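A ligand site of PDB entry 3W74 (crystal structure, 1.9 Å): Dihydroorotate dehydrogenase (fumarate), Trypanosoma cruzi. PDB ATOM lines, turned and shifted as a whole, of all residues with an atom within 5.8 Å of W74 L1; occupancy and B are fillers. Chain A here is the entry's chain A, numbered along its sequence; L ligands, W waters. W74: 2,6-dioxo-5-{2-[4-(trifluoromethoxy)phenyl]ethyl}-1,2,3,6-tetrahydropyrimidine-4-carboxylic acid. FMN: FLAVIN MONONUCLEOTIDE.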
ATOM      1  N   LYS A  44      18.983  17.775 -38.051  1.00  0.00           N
ATOM      2  CA  LYS A  44      19.560  17.951 -36.722  1.00  0.00           C
ATOM      3  C   LYS A  44      21.081  17.908 -36.803  1.00  0.00           C
ATOM      4  O   LYS A  44      21.642  16.964 -37.363  1.00  0.00           O
ATOM      5  CB  LYS A  44      19.053  16.868 -35.771  1.00  0.00           C
ATOM      6  CG  LYS A  44      19.717  16.787 -34.408  1.00  0.00           C
ATOM      7  CD  LYS A  44      19.428  17.986 -33.549  1.00  0.00           C
ATOM      8  CE  LYS A  44      20.421  18.045 -32.417  1.00  0.00           C
ATOM      9  NZ  LYS A  44      20.115  19.146 -31.438  1.00  0.00           N
ATOM     10  N   SER A  45      21.727  18.826 -36.111  1.00  0.00           N
ATOM     11  CA  SER A  45      23.183  18.788 -35.977  1.00  0.00           C
ATOM     12  C   SER A  45      23.654  17.419 -35.468  1.00  0.00           C
ATOM     13  O   SER A  45      23.241  16.971 -34.414  1.00  0.00           O
ATOM     14  CB  SER A  45      23.676  19.847 -35.041  1.00  0.00           C
ATOM     15  OG  SER A  45      23.602  21.084 -35.621  1.00  0.00           O
ATOM     16  N   ASN A  54      21.222  15.232 -23.323  1.00  0.00           N
ATOM     17  CA  ASN A  54      21.122  15.448 -21.893  1.00  0.00           C
ATOM     18  C   ASN A  54      19.838  14.915 -21.227  1.00  0.00           C
ATOM     19  O   ASN A  54      18.856  14.561 -21.908  1.00  0.00           O
ATOM     20  CB  ASN A  54      21.280  16.920 -21.590  1.00  0.00           C
ATOM     21  CG  ASN A  54      22.670  17.418 -21.796  1.00  0.00           C
ATOM     22  OD1 ASN A  54      23.621  16.652 -21.814  1.00  0.00           O
ATOM     23  ND2 ASN A  54      22.801  18.718 -21.989  1.00  0.00           N
ATOM     24  N   ASN A  68      16.860  25.751 -23.747  1.00  0.00           N
ATOM     25  CA  ASN A  68      17.128  24.332 -24.097  1.00  0.00           C
ATOM     26  C   ASN A  68      18.559  23.989 -23.753  1.00  0.00           C
ATOM     27  O   ASN A  68      19.504  24.863 -23.909  1.00  0.00           O
ATOM     28  CB  ASN A  68      16.839  24.042 -25.569  1.00  0.00           C
ATOM     29  CG  ASN A  68      18.043  24.217 -26.441  1.00  0.00           C
ATOM     30  OD1 ASN A  68      18.986  23.362 -26.452  1.00  0.00           O
ATOM     31  ND2 ASN A  68      18.085  25.326 -27.155  1.00  0.00           N
ATOM     32  N   SER A  69      18.758  22.804 -23.217  1.00  0.00           N
ATOM     33  CA  SER A  69      20.131  22.236 -23.175  1.00  0.00           C
ATOM     34  C   SER A  69      20.016  20.830 -23.645  1.00  0.00           C
ATOM     35  O   SER A  69      20.135  19.916 -22.850  1.00  0.00           O
ATOM     36  CB  SER A  69      20.809  22.198 -21.790  1.00  0.00           C
ATOM     37  OG  SER A  69      20.993  23.490 -21.292  1.00  0.00           O
ATOM     38  N   MET A  70      19.774  20.683 -24.931  1.00  0.00           N
ATOM     39  CA  MET A  70      19.524  19.355 -25.491  1.00  0.00           C
ATOM     40  C   MET A  70      20.775  18.434 -25.370  1.00  0.00           C
ATOM     41  O   MET A  70      20.678  17.241 -24.974  1.00  0.00           O
ATOM     42  CB  MET A  70      19.083  19.459 -26.898  1.00  0.00           C
ATOM     43  CG  MET A  70      17.889  20.363 -27.130  1.00  0.00           C
ATOM     44  SD  MET A  70      16.379  19.840 -26.305  1.00  0.00           S
ATOM     45  CE  MET A  70      15.911  18.405 -27.213  1.00  0.00           C
ATOM     46  N   GLY A  71      21.938  18.992 -25.639  1.00  0.00           N
ATOM     47  CA  GLY A  71      23.175  18.160 -25.594  1.00  0.00           C
ATOM     48  C   GLY A  71      23.419  17.297 -26.809  1.00  0.00           C
ATOM     49  O   GLY A  71      23.916  16.176 -26.713  1.00  0.00           O
ATOM     50  N   LEU A  72      22.991  17.795 -27.962  1.00  0.00           N
ATOM     51  CA  LEU A  72      23.184  17.150 -29.235  1.00  0.00           C
ATOM     52  C   LEU A  72      22.673  15.719 -29.328  1.00  0.00           C
ATOM     53  O   LEU A  72      23.392  14.838 -29.804  1.00  0.00           O
ATOM     54  CB  LEU A  72      24.707  17.169 -29.531  1.00  0.00           C
ATOM     55  CG  LEU A  72      25.307  17.724 -30.795  1.00  0.00           C
ATOM     56  CD1 LEU A  72      24.489  18.757 -31.463  1.00  0.00           C
ATOM     57  CD2 LEU A  72      26.705  18.290 -30.465  1.00  0.00           C
ATOM     58  N   PRO A  73      21.444  15.493 -28.904  1.00  0.00           N
ATOM     59  CA  PRO A  73      20.858  14.166 -29.187  1.00  0.00           C
ATOM     60  C   PRO A  73      20.626  14.060 -30.685  1.00  0.00           C
ATOM     61  O   PRO A  73      20.143  15.021 -31.301  1.00  0.00           O
ATOM     62  CB  PRO A  73      19.509  14.191 -28.468  1.00  0.00           C
ATOM     63  CG  PRO A  73      19.116  15.641 -28.445  1.00  0.00           C
ATOM     64  CD  PRO A  73      20.421  16.459 -28.452  1.00  0.00           C
ATOM     65  N   SER A 100      27.941  18.903 -36.231  1.00  0.00           N
ATOM     66  CA  SER A 100      28.409  19.528 -35.011  1.00  0.00           C
ATOM     67  C   SER A 100      29.370  18.606 -34.278  1.00  0.00           C
ATOM     68  O   SER A 100      29.142  18.180 -33.122  1.00  0.00           O
ATOM     69  CB  SER A 100      27.217  19.901 -34.098  1.00  0.00           C
ATOM     70  OG  SER A 100      27.706  20.559 -32.965  1.00  0.00           O
ATOM     71  N   ASN A 128      28.208  23.671 -37.749  1.00  0.00           N
ATOM     72  CA  ASN A 128      27.773  24.318 -36.529  1.00  0.00           C
ATOM     73  C   ASN A 128      28.980  24.670 -35.693  1.00  0.00           C
ATOM     74  O   ASN A 128      29.659  23.786 -35.170  1.00  0.00           O
ATOM     75  CB  ASN A 128      26.840  23.431 -35.729  1.00  0.00           C
ATOM     76  CG  ASN A 128      26.276  24.092 -34.497  1.00  0.00           C
ATOM     77  OD1 ASN A 128      26.641  25.193 -34.113  1.00  0.00           O
ATOM     78  ND2 ASN A 128      25.308  23.413 -33.907  1.00  0.00           N
ATOM     79  N   SER A 130      28.816  26.832 -33.236  1.00  0.00           N
ATOM     80  CA  SER A 130      28.247  27.448 -32.025  1.00  0.00           C
ATOM     81  C   SER A 130      28.118  26.321 -31.070  1.00  0.00           C
ATOM     82  O   SER A 130      27.036  26.037 -30.559  1.00  0.00           O
ATOM     83  CB  SER A 130      26.857  28.086 -32.252  1.00  0.00           C
ATOM     84  OG  SER A 130      26.501  28.241 -33.671  1.00  0.00           O
ATOM     85  N   CYS A 131      29.261  25.705 -30.797  1.00  0.00           N
ATOM     86  CA  CYS A 131      29.378  24.333 -30.376  1.00  0.00           C
ATOM     87  C   CYS A 131      30.677  24.068 -29.512  1.00  0.00           C
ATOM     88  O   CYS A 131      31.773  24.480 -29.935  1.00  0.00           O
ATOM     89  CB  CYS A 131      29.515  23.526 -31.668  1.00  0.00           C
ATOM     90  SG  CYS A 131      30.111  21.838 -31.441  1.00  0.00           S
ATOM     91  N   PRO A 132      30.569  23.333 -28.365  1.00  0.00           N
ATOM     92  CA  PRO A 132      31.682  22.713 -27.582  1.00  0.00           C
ATOM     93  C   PRO A 132      32.992  22.280 -28.265  1.00  0.00           C
ATOM     94  O   PRO A 132      33.000  21.530 -29.266  1.00  0.00           O
ATOM     95  CB  PRO A 132      30.993  21.485 -27.004  1.00  0.00           C
ATOM     96  CG  PRO A 132      29.611  21.991 -26.678  1.00  0.00           C
ATOM     97  CD  PRO A 132      29.316  23.196 -27.590  1.00  0.00           C
ATOM     98  N   ASN A 195      22.637  31.211 -33.683  1.00  0.00           N
ATOM     99  CA  ASN A 195      22.292  30.141 -32.750  1.00  0.00           C
ATOM    100  C   ASN A 195      21.688  30.814 -31.528  1.00  0.00           C
ATOM    101  O   ASN A 195      21.516  32.050 -31.505  1.00  0.00           O
ATOM    102  CB  ASN A 195      23.521  29.265 -32.402  1.00  0.00           C
ATOM    103  CG  ASN A 195      23.169  27.857 -32.180  1.00  0.00           C
ATOM    104  OD1 ASN A 195      22.334  27.555 -31.320  1.00  0.00           O
ATOM    105  ND2 ASN A 195      23.691  26.988 -33.017  1.00  0.00           N
ATOM    106  N   SER A 196      21.330  30.004 -30.521  1.00  0.00           N
ATOM    107  CA  SER A 196      20.680  30.512 -29.328  1.00  0.00           C
ATOM    108  C   SER A 196      21.591  31.464 -28.541  1.00  0.00           C
ATOM    109  O   SER A 196      22.860  31.406 -28.609  1.00  0.00           O
ATOM    110  CB  SER A 196      20.129  29.314 -28.526  1.00  0.00           C
ATOM    111  OG  SER A 196      21.109  28.393 -28.323  1.00  0.00           O
ATOM    112  N   PRO A 214      19.657  19.980 -17.075  1.00  0.00           N
ATOM    113  CA  PRO A 214      21.123  20.014 -17.320  1.00  0.00           C
ATOM    114  C   PRO A 214      21.721  21.336 -16.894  1.00  0.00           C
ATOM    115  O   PRO A 214      21.003  22.318 -16.803  1.00  0.00           O
ATOM    116  CB  PRO A 214      21.197  19.864 -18.842  1.00  0.00           C
ATOM    117  CG  PRO A 214      19.995  19.029 -19.151  1.00  0.00           C
ATOM    118  CD  PRO A 214      18.973  19.823 -18.362  1.00  0.00           C
ATOM    119  N   LYS A 215      23.017  21.376 -16.585  1.00  0.00           N
ATOM    120  CA  LYS A 215      23.704  22.611 -16.309  1.00  0.00           C
ATOM    121  C   LYS A 215      23.051  23.539 -15.275  1.00  0.00           C
ATOM    122  O   LYS A 215      23.122  24.716 -15.392  1.00  0.00           O
ATOM    123  CB  LYS A 215      23.930  23.363 -17.636  1.00  0.00           C
ATOM    124  CG  LYS A 215      24.808  22.567 -18.613  1.00  0.00           C
ATOM    125  CD  LYS A 215      24.919  23.275 -19.958  1.00  0.00           C
ATOM    126  CE  LYS A 215      25.335  24.745 -19.817  1.00  0.00           C
ATOM    127  NZ  LYS A 215      25.687  25.352 -21.143  1.00  0.00           N
ATOM    128  N   GLY A 220      20.411  27.553 -23.665  1.00  0.00           N
ATOM    129  CA  GLY A 220      20.324  28.547 -24.730  1.00  0.00           C
ATOM    130  C   GLY A 220      18.923  29.071 -24.966  1.00  0.00           C
ATOM    131  O   GLY A 220      17.946  28.320 -24.984  1.00  0.00           O
HETATM  132  OAJ W74 L   1      21.756  20.200 -28.927  1.00  0.00           O
HETATM  133  CAI W74 L   1      21.803  21.320 -28.433  1.00  0.00           C
HETATM  134  OAK W74 L   1      21.889  21.429 -27.215  1.00  0.00           O
HETATM  135  C4  W74 L   1      21.943  22.515 -29.187  1.00  0.00           C
HETATM  136  N3  W74 L   1      21.019  23.492 -28.843  1.00  0.00           N
HETATM  137  C2  W74 L   1      21.086  24.739 -29.462  1.00  0.00           C
HETATM  138  O2  W74 L   1      20.324  25.622 -29.106  1.00  0.00           O
HETATM  139  N1  W74 L   1      22.067  24.991 -30.359  1.00  0.00           N
HETATM  140  C6  W74 L   1      23.022  24.038 -30.719  1.00  0.00           C
HETATM  141  O6  W74 L   1      23.895  24.400 -31.521  1.00  0.00           O
HETATM  142  C5  W74 L   1      22.983  22.759 -30.096  1.00  0.00           C
HETATM  143  CAL W74 L   1      23.948  21.791 -30.423  1.00  0.00           C
HETATM  144  CAM W74 L   1      25.405  22.329 -29.998  1.00  0.00           C
HETATM  145  CAN W74 L   1      25.559  22.271 -28.599  1.00  0.00           C
HETATM  146  CAO W74 L   1      25.280  23.389 -27.837  1.00  0.00           C
HETATM  147  CAP W74 L   1      25.369  23.380 -26.425  1.00  0.00           C
HETATM  148  CAQ W74 L   1      25.783  22.212 -25.748  1.00  0.00           C
HETATM  149  OAT W74 L   1      25.892  22.211 -24.337  1.00  0.00           O
HETATM  150  CAU W74 L   1      24.815  21.524 -23.681  1.00  0.00           C
HETATM  151  FAW W74 L   1      24.972  20.266 -23.832  1.00  0.00           F
HETATM  152  FAX W74 L   1      23.568  21.939 -24.209  1.00  0.00           F
HETATM  153  FAV W74 L   1      24.867  21.799 -22.411  1.00  0.00           F
HETATM  154  CAR W74 L   1      26.039  21.079 -26.546  1.00  0.00           C
HETATM  155  CAS W74 L   1      25.942  21.100 -27.951  1.00  0.00           C
HETATM  156  N1  FMN L   2      21.116  24.891 -33.591  1.00  0.00           N
HETATM  157  C2  FMN L   2      21.996  24.153 -34.262  1.00  0.00           C
HETATM  158  O2  FMN L   2      22.704  24.793 -35.079  1.00  0.00           O
HETATM  159  N3  FMN L   2      22.051  22.812 -34.089  1.00  0.00           N
HETATM  160  C4  FMN L   2      21.214  22.084 -33.313  1.00  0.00           C
HETATM  161  O4  FMN L   2      21.198  20.847 -33.166  1.00  0.00           O
HETATM  162  C4A FMN L   2      20.209  22.867 -32.574  1.00  0.00           C
HETATM  163  N5  FMN L   2      19.316  22.295 -31.763  1.00  0.00           N
HETATM  164  C5A FMN L   2      18.290  22.987 -31.189  1.00  0.00           C
HETATM  165  C6  FMN L   2      17.307  22.324 -30.419  1.00  0.00           C
HETATM  166  C7  FMN L   2      16.286  23.060 -29.773  1.00  0.00           C
HETATM  167  C7M FMN L   2      15.233  22.370 -28.904  1.00  0.00           C
HETATM  168  C8  FMN L   2      16.211  24.512 -29.966  1.00  0.00           C
HETATM  169  C8M FMN L   2      15.089  25.226 -29.220  1.00  0.00           C
HETATM  170  C9  FMN L   2      17.160  25.154 -30.761  1.00  0.00           C
HETATM  171  C9A FMN L   2      18.194  24.440 -31.392  1.00  0.00           C
HETATM  172  N10 FMN L   2      19.189  25.026 -32.189  1.00  0.00           N
HETATM  173  C10 FMN L   2      20.191  24.297 -32.805  1.00  0.00           C
HETATM  174  C1' FMN L   2      19.190  26.439 -32.388  1.00  0.00           C
HETATM  175  C2' FMN L   2      18.089  26.884 -33.282  1.00  0.00           C
HETATM  176  O2' FMN L   2      18.532  26.319 -34.498  1.00  0.00           O
HETATM  177  C3' FMN L   2      18.061  28.389 -33.385  1.00  0.00           C
HETATM  178  O3' FMN L   2      19.398  28.791 -33.744  1.00  0.00           O
HETATM  179  C4' FMN L   2      17.654  29.108 -32.098  1.00  0.00           C
HETATM  180  O4' FMN L   2      16.632  28.351 -31.349  1.00  0.00           O
HETATM  181  C5' FMN L   2      17.141  30.527 -32.410  1.00  0.00           C
HETATM  182  O5' FMN L   2      15.979  30.529 -33.241  1.00  0.00           O
HETATM  183  P   FMN L   2      14.479  30.805 -32.675  1.00  0.00           P
HETATM  184  O1P FMN L   2      13.581  30.601 -33.875  1.00  0.00           O
HETATM  185  O2P FMN L   2      14.578  32.079 -31.875  1.00  0.00           O
HETATM  186  O3P FMN L   2      14.298  29.659 -31.735  1.00  0.00           O
HETATM  187  O   HOH W   1      22.018  23.790 -25.619  1.00  0.00           O
HETATM  188  O   HOH W   2      27.123  18.060 -25.219  1.00  0.00           O
HETATM  189  O   HOH W   3      23.122  25.122 -23.637  1.00  0.00           O
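OD1 of Asn 195 lies within hydrogen-bond range of N1 of W74 L1, at 2.8 Å.
N of Leu 72 is in hydrogen-bond range of OAJ of W74 L1, at 2.9 Å.
An oxygen (OAK) of W74 L1 is in hydrogen-bond range of the backbone NH of Gly 71 (2.9 Å).
An oxygen (O6) of W74 L1 is in hydrogen-bond range of the side-chain amide nitrogen (ND2) of Asn 128, at 2.9 Å.
The side-chain amide nitrogen (ND2) of Asn 68 lies within hydrogen-bond range of an oxygen (O2) of W74 L1, 3.0 Å away.
The side-chain hydroxyl (OG) of Ser 196 is in hydrogen-bond range of an oxygen (O2) of W74 L1 (3.0 Å).
The side-chain amino group of Lys 44 lies within salt-bridge range of an oxygen (OAJ) of W74 L1, 3.2 Å away.
N of Met 70 lies within hydrogen-bond range of OAK of W74 L1 (3.2 Å).
O2 of FMN L2 lies within hydrogen-bond range of ND2 of Asn 195, at 3.2 Å.
ND2 of Asn 128 sits at hydrogen-bond distance from O2 of FMN L2 (3.2 Å).
An oxygen (O4) of FMN L2 is in hydrogen-bond range of the side-chain amino group (NZ) of Lys 44, at 2.7 Å.
A nitrogen (N3) of FMN L2 sits at hydrogen-bond distance from the side-chain hydroxyl (OG) of Ser 45.
A nitrogen (N1) of W74 L1 sits close to a nitrogen (N1) of FMN L2 (3.4 Å).
The side-chain hydroxyl (OG) of Ser 196 sits at hydrogen-bond distance from the side-chain amide oxygen (OD1) of Asn 195, 3.3 Å away.
The side-chain amide nitrogen of Asn 195 sits at hydrogen-bond distance from the side-chain hydroxyl of Ser 130 (3.1 Å).
The side-chain amide oxygen of Asn 128 lies within hydrogen-bond range of the backbone NH of Ser 130 (2.9 Å).
The side-chain amide nitrogen (ND2) of Asn 128 lies within hydrogen-bond range of the side-chain hydroxyl (OG) of Ser 45, at 3.4 Å.
The backbone NH (N) of Met 70 lies within hydrogen-bond range of the side-chain amide oxygen (OD1) of Asn 68 (3.2 Å).
The backbone NH of Gly 220 lies within hydrogen-bond range of the backbone carbonyl oxygen of Asn 68 (2.8 Å).
The backbone carbonyl oxygen of Met 70 lies within hydrogen-bond range of the backbone NH of Asn 54 (2.7 Å).
The side-chain amide nitrogen (ND2) of Asn 54 is in hydrogen-bond range of the backbone carbonyl oxygen (O) of Ser 69, 3.0 Å away.
Water W1 lies within hydrogen-bond range of OAK of W74 L1 and OD1 of Asn 68.
ND2 of Asn 54 sits close to FAW of W74 L1 (3.2 Å).
Residues that only touch W74 L1: Lys 215 (2.9 Å), Ser 69 (3.6 Å), Ser 130 (3.7 Å) and Pro 132 (3.7 Å).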
